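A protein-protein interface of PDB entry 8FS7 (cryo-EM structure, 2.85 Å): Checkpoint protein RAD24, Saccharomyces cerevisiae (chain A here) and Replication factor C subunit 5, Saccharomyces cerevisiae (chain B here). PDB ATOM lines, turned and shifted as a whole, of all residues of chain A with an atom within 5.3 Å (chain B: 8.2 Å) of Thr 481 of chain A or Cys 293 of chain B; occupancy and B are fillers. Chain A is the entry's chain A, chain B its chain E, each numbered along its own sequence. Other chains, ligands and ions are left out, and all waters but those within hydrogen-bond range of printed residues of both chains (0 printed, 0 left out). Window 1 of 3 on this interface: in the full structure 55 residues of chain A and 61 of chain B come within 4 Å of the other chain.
NE2 of Gln 453 of chain A is in hydrogen-bond range of O of Leu 290 of chain B, at 2.7 Å. The guanidinium group of Arg 538 of chain A is in salt-bridge range of the side-chain carboxylate of Asp 258 of chain B. The backbone carbonyl oxygen of Gln 453 of chain A is in hydrogen-bond range of the side-chain sulfur of Cys 293 of chain B. The backbone carbonyl oxygen (O) of Leu 482 of chain A sits at hydrogen-bond distance from the indole nitrogen (NE1) of Trp 259 of chain B.
The side-chain hydroxyl (OG1) of Thr 481 of chain A sits at hydrogen-bond distance from the backbone carbonyl oxygen (O) of Arg 478 of chain A.
CB of Leu 452 of chain A touches CB of Ala 291 of chain B (3.7 Å). Ala 291 of chain B touches Gln 453 of chain A. His 292 of chain B touches Phe 456 of chain A. Phe 456 of chain A touches Cys 293 of chain B (CD1 to CB, 3.5 Å). Arg 478 of chain A touches Pro 295 of chain B (NH1 to CG, 3.3 Å). Ile 298 of chain B touches Arg 478 of chain A. CB of Thr 481 of chain A touches O of Cys 293 of chain B, at 3.3 Å. Leu 482 of chain A touches Ile 298 of chain B.
Of the printed residues of chain B, Arg 478 of chain A touches Pro 295 (3.3 Å) and Ile 298 (3.3 Å). Thr 481 of chain A touches just one residue of chain B: Cys 293 (3.3 Å). Of the printed residues of chain B, Leu 482 of chain A touches Trp 259 and Ile 298. Printed residues of chain A within 4 Å of Asp 258 of chain B: Arg 538. Of the printed residues of chain A, Leu 290 of chain B touches Gln 453. Printed residues of chain A within 4 Å of Cys 293 of chain B: Gln 453 (3.6 Å), Phe 456 (3.5 Å) and Thr 481 (3.3 Å).
Of the 15 printed residues of chain A, 7 touch a printed residue of chain B. Of the 16 printed residues of chain B, 8 touch a printed residue of chain A. Among the printed residues, Asp or Glu carboxylates within 4 Å of a Lys or Arg side-chain nitrogen of the other chain: Arg 538 of chain A with Asp 258 of chain B.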
ATOM      1  N   LEU A 452      16.257 -20.460 -29.647  1.00  0.00           N
ATOM      2  CA  LEU A 452      15.732 -19.152 -29.270  1.00  0.00           C
ATOM      3  C   LEU A 452      16.437 -18.614 -28.030  1.00  0.00           C
ATOM      4  O   LEU A 452      16.716 -17.413 -27.937  1.00  0.00           O
ATOM      5  CB  LEU A 452      14.224 -19.237 -29.040  1.00  0.00           C
ATOM      6  CG  LEU A 452      13.347 -19.180 -30.293  1.00  0.00           C
ATOM      7  CD1 LEU A 452      12.028 -19.902 -30.061  1.00  0.00           C
ATOM      8  CD2 LEU A 452      13.106 -17.739 -30.715  1.00  0.00           C
ATOM      9  N   GLN A 453      16.731 -19.491 -27.068  1.00  0.00           N
ATOM     10  CA  GLN A 453      17.468 -19.076 -25.879  1.00  0.00           C
ATOM     11  C   GLN A 453      18.886 -18.644 -26.228  1.00  0.00           C
ATOM     12  O   GLN A 453      19.416 -17.704 -25.629  1.00  0.00           O
ATOM     13  CB  GLN A 453      17.489 -20.207 -24.850  1.00  0.00           C
ATOM     14  CG  GLN A 453      16.177 -20.391 -24.104  1.00  0.00           C
ATOM     15  CD  GLN A 453      16.112 -21.708 -23.357  1.00  0.00           C
ATOM     16  OE1 GLN A 453      16.940 -22.594 -23.564  1.00  0.00           O
ATOM     17  NE2 GLN A 453      15.122 -21.843 -22.483  1.00  0.00           N
ATOM     18  N   PHE A 456      18.574 -15.207 -27.673  1.00  0.00           N
ATOM     19  CA  PHE A 456      18.352 -14.286 -26.564  1.00  0.00           C
ATOM     20  C   PHE A 456      19.647 -14.024 -25.807  1.00  0.00           C
ATOM     21  O   PHE A 456      19.908 -12.894 -25.383  1.00  0.00           O
ATOM     22  CB  PHE A 456      17.279 -14.853 -25.629  1.00  0.00           C
ATOM     23  CG  PHE A 456      16.754 -13.866 -24.616  1.00  0.00           C
ATOM     24  CD1 PHE A 456      17.477 -13.561 -23.473  1.00  0.00           C
ATOM     25  CD2 PHE A 456      15.521 -13.262 -24.800  1.00  0.00           C
ATOM     26  CE1 PHE A 456      16.989 -12.661 -22.545  1.00  0.00           C
ATOM     27  CE2 PHE A 456      15.027 -12.365 -23.872  1.00  0.00           C
ATOM     28  CZ  PHE A 456      15.763 -12.063 -22.744  1.00  0.00           C
ATOM     29  N   LYS A 457      20.466 -15.062 -25.620  1.00  0.00           N
ATOM     30  CA  LYS A 457      21.751 -14.899 -24.949  1.00  0.00           C
ATOM     31  C   LYS A 457      22.669 -13.974 -25.734  1.00  0.00           C
ATOM     32  O   LYS A 457      23.341 -13.117 -25.152  1.00  0.00           O
ATOM     33  CB  LYS A 457      22.413 -16.263 -24.752  1.00  0.00           C
ATOM     34  CG  LYS A 457      22.022 -16.979 -23.471  1.00  0.00           C
ATOM     35  CD  LYS A 457      22.635 -16.309 -22.253  1.00  0.00           C
ATOM     36  CE  LYS A 457      22.694 -17.266 -21.074  1.00  0.00           C
ATOM     37  NZ  LYS A 457      21.371 -17.888 -20.794  1.00  0.00           N
ATOM     38  N   SER A 476      22.822  -7.556 -14.317  1.00  0.00           N
ATOM     39  CA  SER A 476      22.877  -9.009 -14.359  1.00  0.00           C
ATOM     40  C   SER A 476      21.962  -9.535 -15.456  1.00  0.00           C
ATOM     41  O   SER A 476      20.937  -8.923 -15.773  1.00  0.00           O
ATOM     42  CB  SER A 476      22.481  -9.612 -13.011  1.00  0.00           C
ATOM     43  OG  SER A 476      21.337  -8.969 -12.479  1.00  0.00           O
ATOM     44  N   PHE A 477      22.349 -10.678 -16.033  1.00  0.00           N
ATOM     45  CA  PHE A 477      21.534 -11.318 -17.061  1.00  0.00           C
ATOM     46  C   PHE A 477      20.143 -11.649 -16.536  1.00  0.00           C
ATOM     47  O   PHE A 477      19.165 -11.637 -17.291  1.00  0.00           O
ATOM     48  CB  PHE A 477      22.240 -12.579 -17.565  1.00  0.00           C
ATOM     49  CG  PHE A 477      21.443 -13.370 -18.561  1.00  0.00           C
ATOM     50  CD1 PHE A 477      21.249 -12.898 -19.849  1.00  0.00           C
ATOM     51  CD2 PHE A 477      20.896 -14.595 -18.213  1.00  0.00           C
ATOM     52  CE1 PHE A 477      20.519 -13.630 -20.767  1.00  0.00           C
ATOM     53  CE2 PHE A 477      20.166 -15.330 -19.127  1.00  0.00           C
ATOM     54  CZ  PHE A 477      19.978 -14.847 -20.406  1.00  0.00           C
ATOM     55  N   ARG A 478      20.039 -11.933 -15.237  1.00  0.00           N
ATOM     56  CA  ARG A 478      18.740 -12.158 -14.611  1.00  0.00           C
ATOM     57  C   ARG A 478      17.849 -10.925 -14.751  1.00  0.00           C
ATOM     58  O   ARG A 478      16.675 -11.026 -15.130  1.00  0.00           O
ATOM     59  CB  ARG A 478      18.958 -12.527 -13.140  1.00  0.00           C
ATOM     60  CG  ARG A 478      17.916 -12.014 -12.167  1.00  0.00           C
ATOM     61  CD  ARG A 478      16.708 -12.920 -12.140  1.00  0.00           C
ATOM     62  NE  ARG A 478      17.050 -14.265 -11.692  1.00  0.00           N
ATOM     63  CZ  ARG A 478      16.158 -15.198 -11.393  1.00  0.00           C
ATOM     64  NH1 ARG A 478      14.859 -14.955 -11.458  1.00  0.00           N
ATOM     65  NH2 ARG A 478      16.578 -16.400 -11.012  1.00  0.00           N
ATOM     66  N   ASN A 479      18.409  -9.743 -14.477  1.00  0.00           N
ATOM     67  CA  ASN A 479      17.664  -8.502 -14.655  1.00  0.00           C
ATOM     68  C   ASN A 479      17.411  -8.196 -16.124  1.00  0.00           C
ATOM     69  O   ASN A 479      16.407  -7.551 -16.450  1.00  0.00           O
ATOM     70  CB  ASN A 479      18.409  -7.338 -14.000  1.00  0.00           C
ATOM     71  CG  ASN A 479      18.613  -7.539 -12.512  1.00  0.00           C
ATOM     72  OD1 ASN A 479      18.015  -8.427 -11.906  1.00  0.00           O
ATOM     73  ND2 ASN A 479      19.464  -6.712 -11.916  1.00  0.00           N
ATOM     74  N   ILE A 480      18.304  -8.632 -17.016  1.00  0.00           N
ATOM     75  CA  ILE A 480      18.065  -8.455 -18.448  1.00  0.00           C
ATOM     76  C   ILE A 480      16.834  -9.241 -18.880  1.00  0.00           C
ATOM     77  O   ILE A 480      15.971  -8.732 -19.604  1.00  0.00           O
ATOM     78  CB  ILE A 480      19.304  -8.862 -19.265  1.00  0.00           C
ATOM     79  CG1 ILE A 480      20.552  -8.126 -18.776  1.00  0.00           C
ATOM     80  CG2 ILE A 480      19.079  -8.592 -20.745  1.00  0.00           C
ATOM     81  CD1 ILE A 480      20.388  -6.627 -18.697  1.00  0.00           C
ATOM     82  N   THR A 481      16.734 -10.498 -18.442  1.00  0.00           N
ATOM     83  CA  THR A 481      15.576 -11.308 -18.815  1.00  0.00           C
ATOM     84  C   THR A 481      14.303 -10.828 -18.128  1.00  0.00           C
ATOM     85  O   THR A 481      13.220 -10.880 -18.725  1.00  0.00           O
ATOM     86  CB  THR A 481      15.815 -12.787 -18.504  1.00  0.00           C
ATOM     87  OG1 THR A 481      15.682 -13.020 -17.096  1.00  0.00           O
ATOM     88  CG2 THR A 481      17.173 -13.242 -18.998  1.00  0.00           C
ATOM     89  N   LEU A 482      14.397 -10.361 -16.881  1.00  0.00           N
ATOM     90  CA  LEU A 482      13.171  -9.983 -16.184  1.00  0.00           C
ATOM     91  C   LEU A 482      12.607  -8.664 -16.700  1.00  0.00           C
ATOM     92  O   LEU A 482      11.498  -8.623 -17.242  1.00  0.00           O
ATOM     93  CB  LEU A 482      13.401  -9.886 -14.674  1.00  0.00           C
ATOM     94  CG  LEU A 482      13.195 -11.131 -13.808  1.00  0.00           C
ATOM     95  CD1 LEU A 482      13.685 -12.403 -14.494  1.00  0.00           C
ATOM     96  CD2 LEU A 482      13.820 -10.946 -12.435  1.00  0.00           C
ATOM     97  N   GLU A 483      13.362  -7.578 -16.546  1.00  0.00           N
ATOM     98  CA  GLU A 483      12.839  -6.238 -16.776  1.00  0.00           C
ATOM     99  C   GLU A 483      13.527  -5.521 -17.925  1.00  0.00           C
ATOM    100  O   GLU A 483      12.853  -4.881 -18.740  1.00  0.00           O
ATOM    101  CB  GLU A 483      12.966  -5.411 -15.488  1.00  0.00           C
ATOM    102  CG  GLU A 483      12.550  -6.163 -14.233  1.00  0.00           C
ATOM    103  CD  GLU A 483      13.562  -6.031 -13.112  1.00  0.00           C
ATOM    104  OE1 GLU A 483      14.547  -5.283 -13.285  1.00  0.00           O
ATOM    105  OE2 GLU A 483      13.372  -6.675 -12.059  1.00  0.00           O
ATOM    106  N   PHE A 484      14.856  -5.609 -18.016  1.00  0.00           N
ATOM    107  CA  PHE A 484      15.591  -4.872 -19.036  1.00  0.00           C
ATOM    108  C   PHE A 484      15.376  -5.417 -20.441  1.00  0.00           C
ATOM    109  O   PHE A 484      15.726  -4.734 -21.408  1.00  0.00           O
ATOM    110  CB  PHE A 484      17.082  -4.868 -18.699  1.00  0.00           C
ATOM    111  CG  PHE A 484      17.439  -3.964 -17.555  1.00  0.00           C
ATOM    112  CD1 PHE A 484      16.699  -2.821 -17.304  1.00  0.00           C
ATOM    113  CD2 PHE A 484      18.509  -4.258 -16.727  1.00  0.00           C
ATOM    114  CE1 PHE A 484      17.020  -1.985 -16.253  1.00  0.00           C
ATOM    115  CE2 PHE A 484      18.834  -3.427 -15.673  1.00  0.00           C
ATOM    116  CZ  PHE A 484      18.090  -2.288 -15.436  1.00  0.00           C
ATOM    117  N   GLY A 485      14.816  -6.620 -20.582  1.00  0.00           N
ATOM    118  CA  GLY A 485      14.503  -7.130 -21.903  1.00  0.00           C
ATOM    119  C   GLY A 485      13.280  -6.498 -22.530  1.00  0.00           C
ATOM    120  O   GLY A 485      13.107  -6.586 -23.750  1.00  0.00           O
ATOM    121  N   ARG A 538      12.503  -5.432 -28.577  1.00  0.00           N
ATOM    122  CA  ARG A 538      12.488  -6.333 -27.433  1.00  0.00           C
ATOM    123  C   ARG A 538      13.474  -7.474 -27.651  1.00  0.00           C
ATOM    124  O   ARG A 538      13.517  -8.077 -28.727  1.00  0.00           O
ATOM    125  CB  ARG A 538      11.077  -6.883 -27.216  1.00  0.00           C
ATOM    126  CG  ARG A 538      10.666  -7.003 -25.758  1.00  0.00           C
ATOM    127  CD  ARG A 538       9.694  -8.154 -25.545  1.00  0.00           C
ATOM    128  NE  ARG A 538       9.606  -8.551 -24.145  1.00  0.00           N
ATOM    129  CZ  ARG A 538      10.505  -9.296 -23.517  1.00  0.00           C
ATOM    130  NH1 ARG A 538      11.577  -9.758 -24.138  1.00  0.00           N
ATOM    131  NH2 ARG A 538      10.323  -9.586 -22.232  1.00  0.00           N
ATOM    132  N   PRO B 257       5.613  -5.679 -17.020  1.00  0.00           N
ATOM    133  CA  PRO B 257       6.419  -6.468 -17.958  1.00  0.00           C
ATOM    134  C   PRO B 257       5.561  -7.383 -18.820  1.00  0.00           C
ATOM    135  O   PRO B 257       4.479  -7.819 -18.418  1.00  0.00           O
ATOM    136  CB  PRO B 257       7.346  -7.274 -17.040  1.00  0.00           C
ATOM    137  CG  PRO B 257       7.443  -6.454 -15.803  1.00  0.00           C
ATOM    138  CD  PRO B 257       6.090  -5.826 -15.633  1.00  0.00           C
ATOM    139  N   ASP B 258       6.057  -7.652 -20.031  1.00  0.00           N
ATOM    140  CA  ASP B 258       5.291  -8.427 -21.002  1.00  0.00           C
ATOM    141  C   ASP B 258       5.024  -9.842 -20.504  1.00  0.00           C
ATOM    142  O   ASP B 258       3.924 -10.377 -20.694  1.00  0.00           O
ATOM    143  CB  ASP B 258       6.030  -8.460 -22.340  1.00  0.00           C
ATOM    144  CG  ASP B 258       5.149  -8.920 -23.485  1.00  0.00           C
ATOM    145  OD1 ASP B 258       3.921  -9.039 -23.283  1.00  0.00           O
ATOM    146  OD2 ASP B 258       5.682  -9.163 -24.587  1.00  0.00           O
ATOM    147  N   TRP B 259       6.018 -10.470 -19.869  1.00  0.00           N
ATOM    148  CA  TRP B 259       5.816 -11.830 -19.383  1.00  0.00           C
ATOM    149  C   TRP B 259       4.831 -11.870 -18.221  1.00  0.00           C
ATOM    150  O   TRP B 259       4.156 -12.885 -18.027  1.00  0.00           O
ATOM    151  CB  TRP B 259       7.154 -12.469 -19.000  1.00  0.00           C
ATOM    152  CG  TRP B 259       7.971 -11.718 -17.992  1.00  0.00           C
ATOM    153  CD1 TRP B 259       8.684 -10.574 -18.200  1.00  0.00           C
ATOM    154  CD2 TRP B 259       8.199 -12.090 -16.627  1.00  0.00           C
ATOM    155  NE1 TRP B 259       9.323 -10.197 -17.044  1.00  0.00           N
ATOM    156  CE2 TRP B 259       9.043 -11.112 -16.064  1.00  0.00           C
ATOM    157  CE3 TRP B 259       7.764 -13.149 -15.824  1.00  0.00           C
ATOM    158  CZ2 TRP B 259       9.459 -11.160 -14.735  1.00  0.00           C
ATOM    159  CZ3 TRP B 259       8.177 -13.195 -14.505  1.00  0.00           C
ATOM    160  CH2 TRP B 259       9.016 -12.206 -13.974  1.00  0.00           C
ATOM    161  N   LEU B 286       4.134 -21.805 -22.056  1.00  0.00           N
ATOM    162  CA  LEU B 286       5.298 -22.061 -21.213  1.00  0.00           C
ATOM    163  C   LEU B 286       6.563 -22.203 -22.047  1.00  0.00           C
ATOM    164  O   LEU B 286       7.641 -21.766 -21.630  1.00  0.00           O
ATOM    165  CB  LEU B 286       5.077 -23.319 -20.374  1.00  0.00           C
ATOM    166  CG  LEU B 286       4.031 -23.266 -19.262  1.00  0.00           C
ATOM    167  CD1 LEU B 286       3.796 -24.662 -18.716  1.00  0.00           C
ATOM    168  CD2 LEU B 286       4.462 -22.316 -18.156  1.00  0.00           C
ATOM    169  N   TYR B 287       6.456 -22.828 -23.220  1.00  0.00           N
ATOM    170  CA  TYR B 287       7.611 -22.965 -24.099  1.00  0.00           C
ATOM    171  C   TYR B 287       8.072 -21.610 -24.618  1.00  0.00           C
ATOM    172  O   TYR B 287       9.276 -21.359 -24.722  1.00  0.00           O
ATOM    173  CB  TYR B 287       7.282 -23.903 -25.259  1.00  0.00           C
ATOM    174  CG  TYR B 287       7.671 -25.341 -25.004  1.00  0.00           C
ATOM    175  CD1 TYR B 287       8.934 -25.663 -24.525  1.00  0.00           C
ATOM    176  CD2 TYR B 287       6.778 -26.377 -25.244  1.00  0.00           C
ATOM    177  CE1 TYR B 287       9.297 -26.974 -24.291  1.00  0.00           C
ATOM    178  CE2 TYR B 287       7.132 -27.692 -25.013  1.00  0.00           C
ATOM    179  CZ  TYR B 287       8.392 -27.985 -24.536  1.00  0.00           C
ATOM    180  OH  TYR B 287       8.749 -29.293 -24.304  1.00  0.00           O
ATOM    181  N   ASP B 288       7.128 -20.726 -24.950  1.00  0.00           N
ATOM    182  CA  ASP B 288       7.493 -19.367 -25.346  1.00  0.00           C
ATOM    183  C   ASP B 288       8.201 -18.637 -24.209  1.00  0.00           C
ATOM    184  O   ASP B 288       9.226 -17.973 -24.418  1.00  0.00           O
ATOM    185  CB  ASP B 288       6.246 -18.599 -25.788  1.00  0.00           C
ATOM    186  CG  ASP B 288       6.535 -17.609 -26.899  1.00  0.00           C
ATOM    187  OD1 ASP B 288       7.594 -17.734 -27.550  1.00  0.00           O
ATOM    188  OD2 ASP B 288       5.703 -16.705 -27.122  1.00  0.00           O
ATOM    189  N   LEU B 289       7.670 -18.764 -22.990  1.00  0.00           N
ATOM    190  CA  LEU B 289       8.291 -18.114 -21.837  1.00  0.00           C
ATOM    191  C   LEU B 289       9.692 -18.657 -21.581  1.00  0.00           C
ATOM    192  O   LEU B 289      10.611 -17.896 -21.255  1.00  0.00           O
ATOM    193  CB  LEU B 289       7.411 -18.290 -20.599  1.00  0.00           C
ATOM    194  CG  LEU B 289       6.084 -17.529 -20.583  1.00  0.00           C
ATOM    195  CD1 LEU B 289       5.128 -18.140 -19.571  1.00  0.00           C
ATOM    196  CD2 LEU B 289       6.313 -16.056 -20.285  1.00  0.00           C
ATOM    197  N   LEU B 290       9.873 -19.974 -21.714  1.00  0.00           N
ATOM    198  CA  LEU B 290      11.193 -20.573 -21.552  1.00  0.00           C
ATOM    199  C   LEU B 290      12.152 -20.107 -22.641  1.00  0.00           C
ATOM    200  O   LEU B 290      13.327 -19.839 -22.367  1.00  0.00           O
ATOM    201  CB  LEU B 290      11.081 -22.098 -21.555  1.00  0.00           C
ATOM    202  CG  LEU B 290      11.145 -22.822 -20.208  1.00  0.00           C
ATOM    203  CD1 LEU B 290      10.279 -22.128 -19.169  1.00  0.00           C
ATOM    204  CD2 LEU B 290      10.733 -24.278 -20.365  1.00  0.00           C
ATOM    205  N   ALA B 291      11.669 -20.013 -23.882  1.00  0.00           N
ATOM    206  CA  ALA B 291      12.488 -19.510 -24.977  1.00  0.00           C
ATOM    207  C   ALA B 291      12.863 -18.049 -24.785  1.00  0.00           C
ATOM    208  O   ALA B 291      13.871 -17.602 -25.343  1.00  0.00           O
ATOM    209  CB  ALA B 291      11.756 -19.691 -26.308  1.00  0.00           C
ATOM    210  N   HIS B 292      12.080 -17.296 -24.013  1.00  0.00           N
ATOM    211  CA  HIS B 292      12.438 -15.932 -23.653  1.00  0.00           C
ATOM    212  C   HIS B 292      13.392 -15.870 -22.460  1.00  0.00           C
ATOM    213  O   HIS B 292      13.561 -14.796 -21.869  1.00  0.00           O
ATOM    214  CB  HIS B 292      11.176 -15.116 -23.375  1.00  0.00           C
ATOM    215  CG  HIS B 292      10.512 -14.601 -24.613  1.00  0.00           C
ATOM    216  ND1 HIS B 292      11.168 -13.814 -25.535  1.00  0.00           N
ATOM    217  CD2 HIS B 292       9.259 -14.778 -25.094  1.00  0.00           C
ATOM    218  CE1 HIS B 292      10.343 -13.518 -26.524  1.00  0.00           C
ATOM    219  NE2 HIS B 292       9.178 -14.091 -26.279  1.00  0.00           N
ATOM    220  N   CYS B 293      14.007 -17.001 -22.098  1.00  0.00           N
ATOM    221  CA  CYS B 293      15.071 -17.070 -21.092  1.00  0.00           C
ATOM    222  C   CYS B 293      14.614 -16.577 -19.721  1.00  0.00           C
ATOM    223  O   CYS B 293      15.390 -15.993 -18.963  1.00  0.00           O
ATOM    224  CB  CYS B 293      16.316 -16.306 -21.547  1.00  0.00           C
ATOM    225  SG  CYS B 293      17.281 -17.138 -22.824  1.00  0.00           S
ATOM    226  N   ILE B 294      13.354 -16.821 -19.388  1.00  0.00           N
ATOM    227  CA  ILE B 294      12.820 -16.531 -18.060  1.00  0.00           C
ATOM    228  C   ILE B 294      12.955 -17.797 -17.222  1.00  0.00           C
ATOM    229  O   ILE B 294      12.476 -18.859 -17.651  1.00  0.00           O
ATOM    230  CB  ILE B 294      11.360 -16.058 -18.121  1.00  0.00           C
ATOM    231  CG1 ILE B 294      11.247 -14.784 -18.957  1.00  0.00           C
ATOM    232  CG2 ILE B 294      10.840 -15.781 -16.724  1.00  0.00           C
ATOM    233  CD1 ILE B 294      10.067 -14.778 -19.900  1.00  0.00           C
ATOM    234  N   PRO B 295      13.608 -17.745 -16.060  1.00  0.00           N
ATOM    235  CA  PRO B 295      13.795 -18.964 -15.259  1.00  0.00           C
ATOM    236  C   PRO B 295      12.464 -19.567 -14.830  1.00  0.00           C
ATOM    237  O   PRO B 295      11.511 -18.857 -14.511  1.00  0.00           O
ATOM    238  CB  PRO B 295      14.609 -18.478 -14.053  1.00  0.00           C
ATOM    239  CG  PRO B 295      14.412 -16.998 -14.018  1.00  0.00           C
ATOM    240  CD  PRO B 295      14.233 -16.567 -15.437  1.00  0.00           C
ATOM    241  N   ALA B 296      12.418 -20.901 -14.817  1.00  0.00           N
ATOM    242  CA  ALA B 296      11.154 -21.600 -14.606  1.00  0.00           C
ATOM    243  C   ALA B 296      10.682 -21.520 -13.159  1.00  0.00           C
ATOM    244  O   ALA B 296       9.478 -21.635 -12.901  1.00  0.00           O
ATOM    245  CB  ALA B 296      11.283 -23.058 -15.037  1.00  0.00           C
ATOM    246  N   ILE B 298      10.766 -18.845 -11.114  1.00  0.00           N
ATOM    247  CA  ILE B 298       9.959 -17.641 -10.968  1.00  0.00           C
ATOM    248  C   ILE B 298       8.731 -17.691 -11.870  1.00  0.00           C
ATOM    249  O   ILE B 298       7.718 -17.055 -11.566  1.00  0.00           O
ATOM    250  CB  ILE B 298      10.807 -16.384 -11.227  1.00  0.00           C
ATOM    251  CG1 ILE B 298      11.035 -16.178 -12.723  1.00  0.00           C
ATOM    252  CG2 ILE B 298      12.125 -16.478 -10.479  1.00  0.00           C
ATOM    253  CD1 ILE B 298      11.389 -14.767 -13.086  1.00  0.00           C
ATOM    254  N   ILE B 299       8.781 -18.448 -12.969  1.00  0.00           N
ATOM    255  CA  ILE B 299       7.578 -18.661 -13.774  1.00  0.00           C
ATOM    256  C   ILE B 299       6.519 -19.376 -12.947  1.00  0.00           C
ATOM    257  O   ILE B 299       5.349 -18.973 -12.915  1.00  0.00           O
ATOM    258  CB  ILE B 299       7.916 -19.447 -15.054  1.00  0.00           C
ATOM    259  CG1 ILE B 299       8.719 -18.577 -16.019  1.00  0.00           C
ATOM    260  CG2 ILE B 299       6.648 -19.962 -15.721  1.00  0.00           C
ATOM    261  CD1 ILE B 299       8.912 -19.191 -17.384  1.00  0.00           C
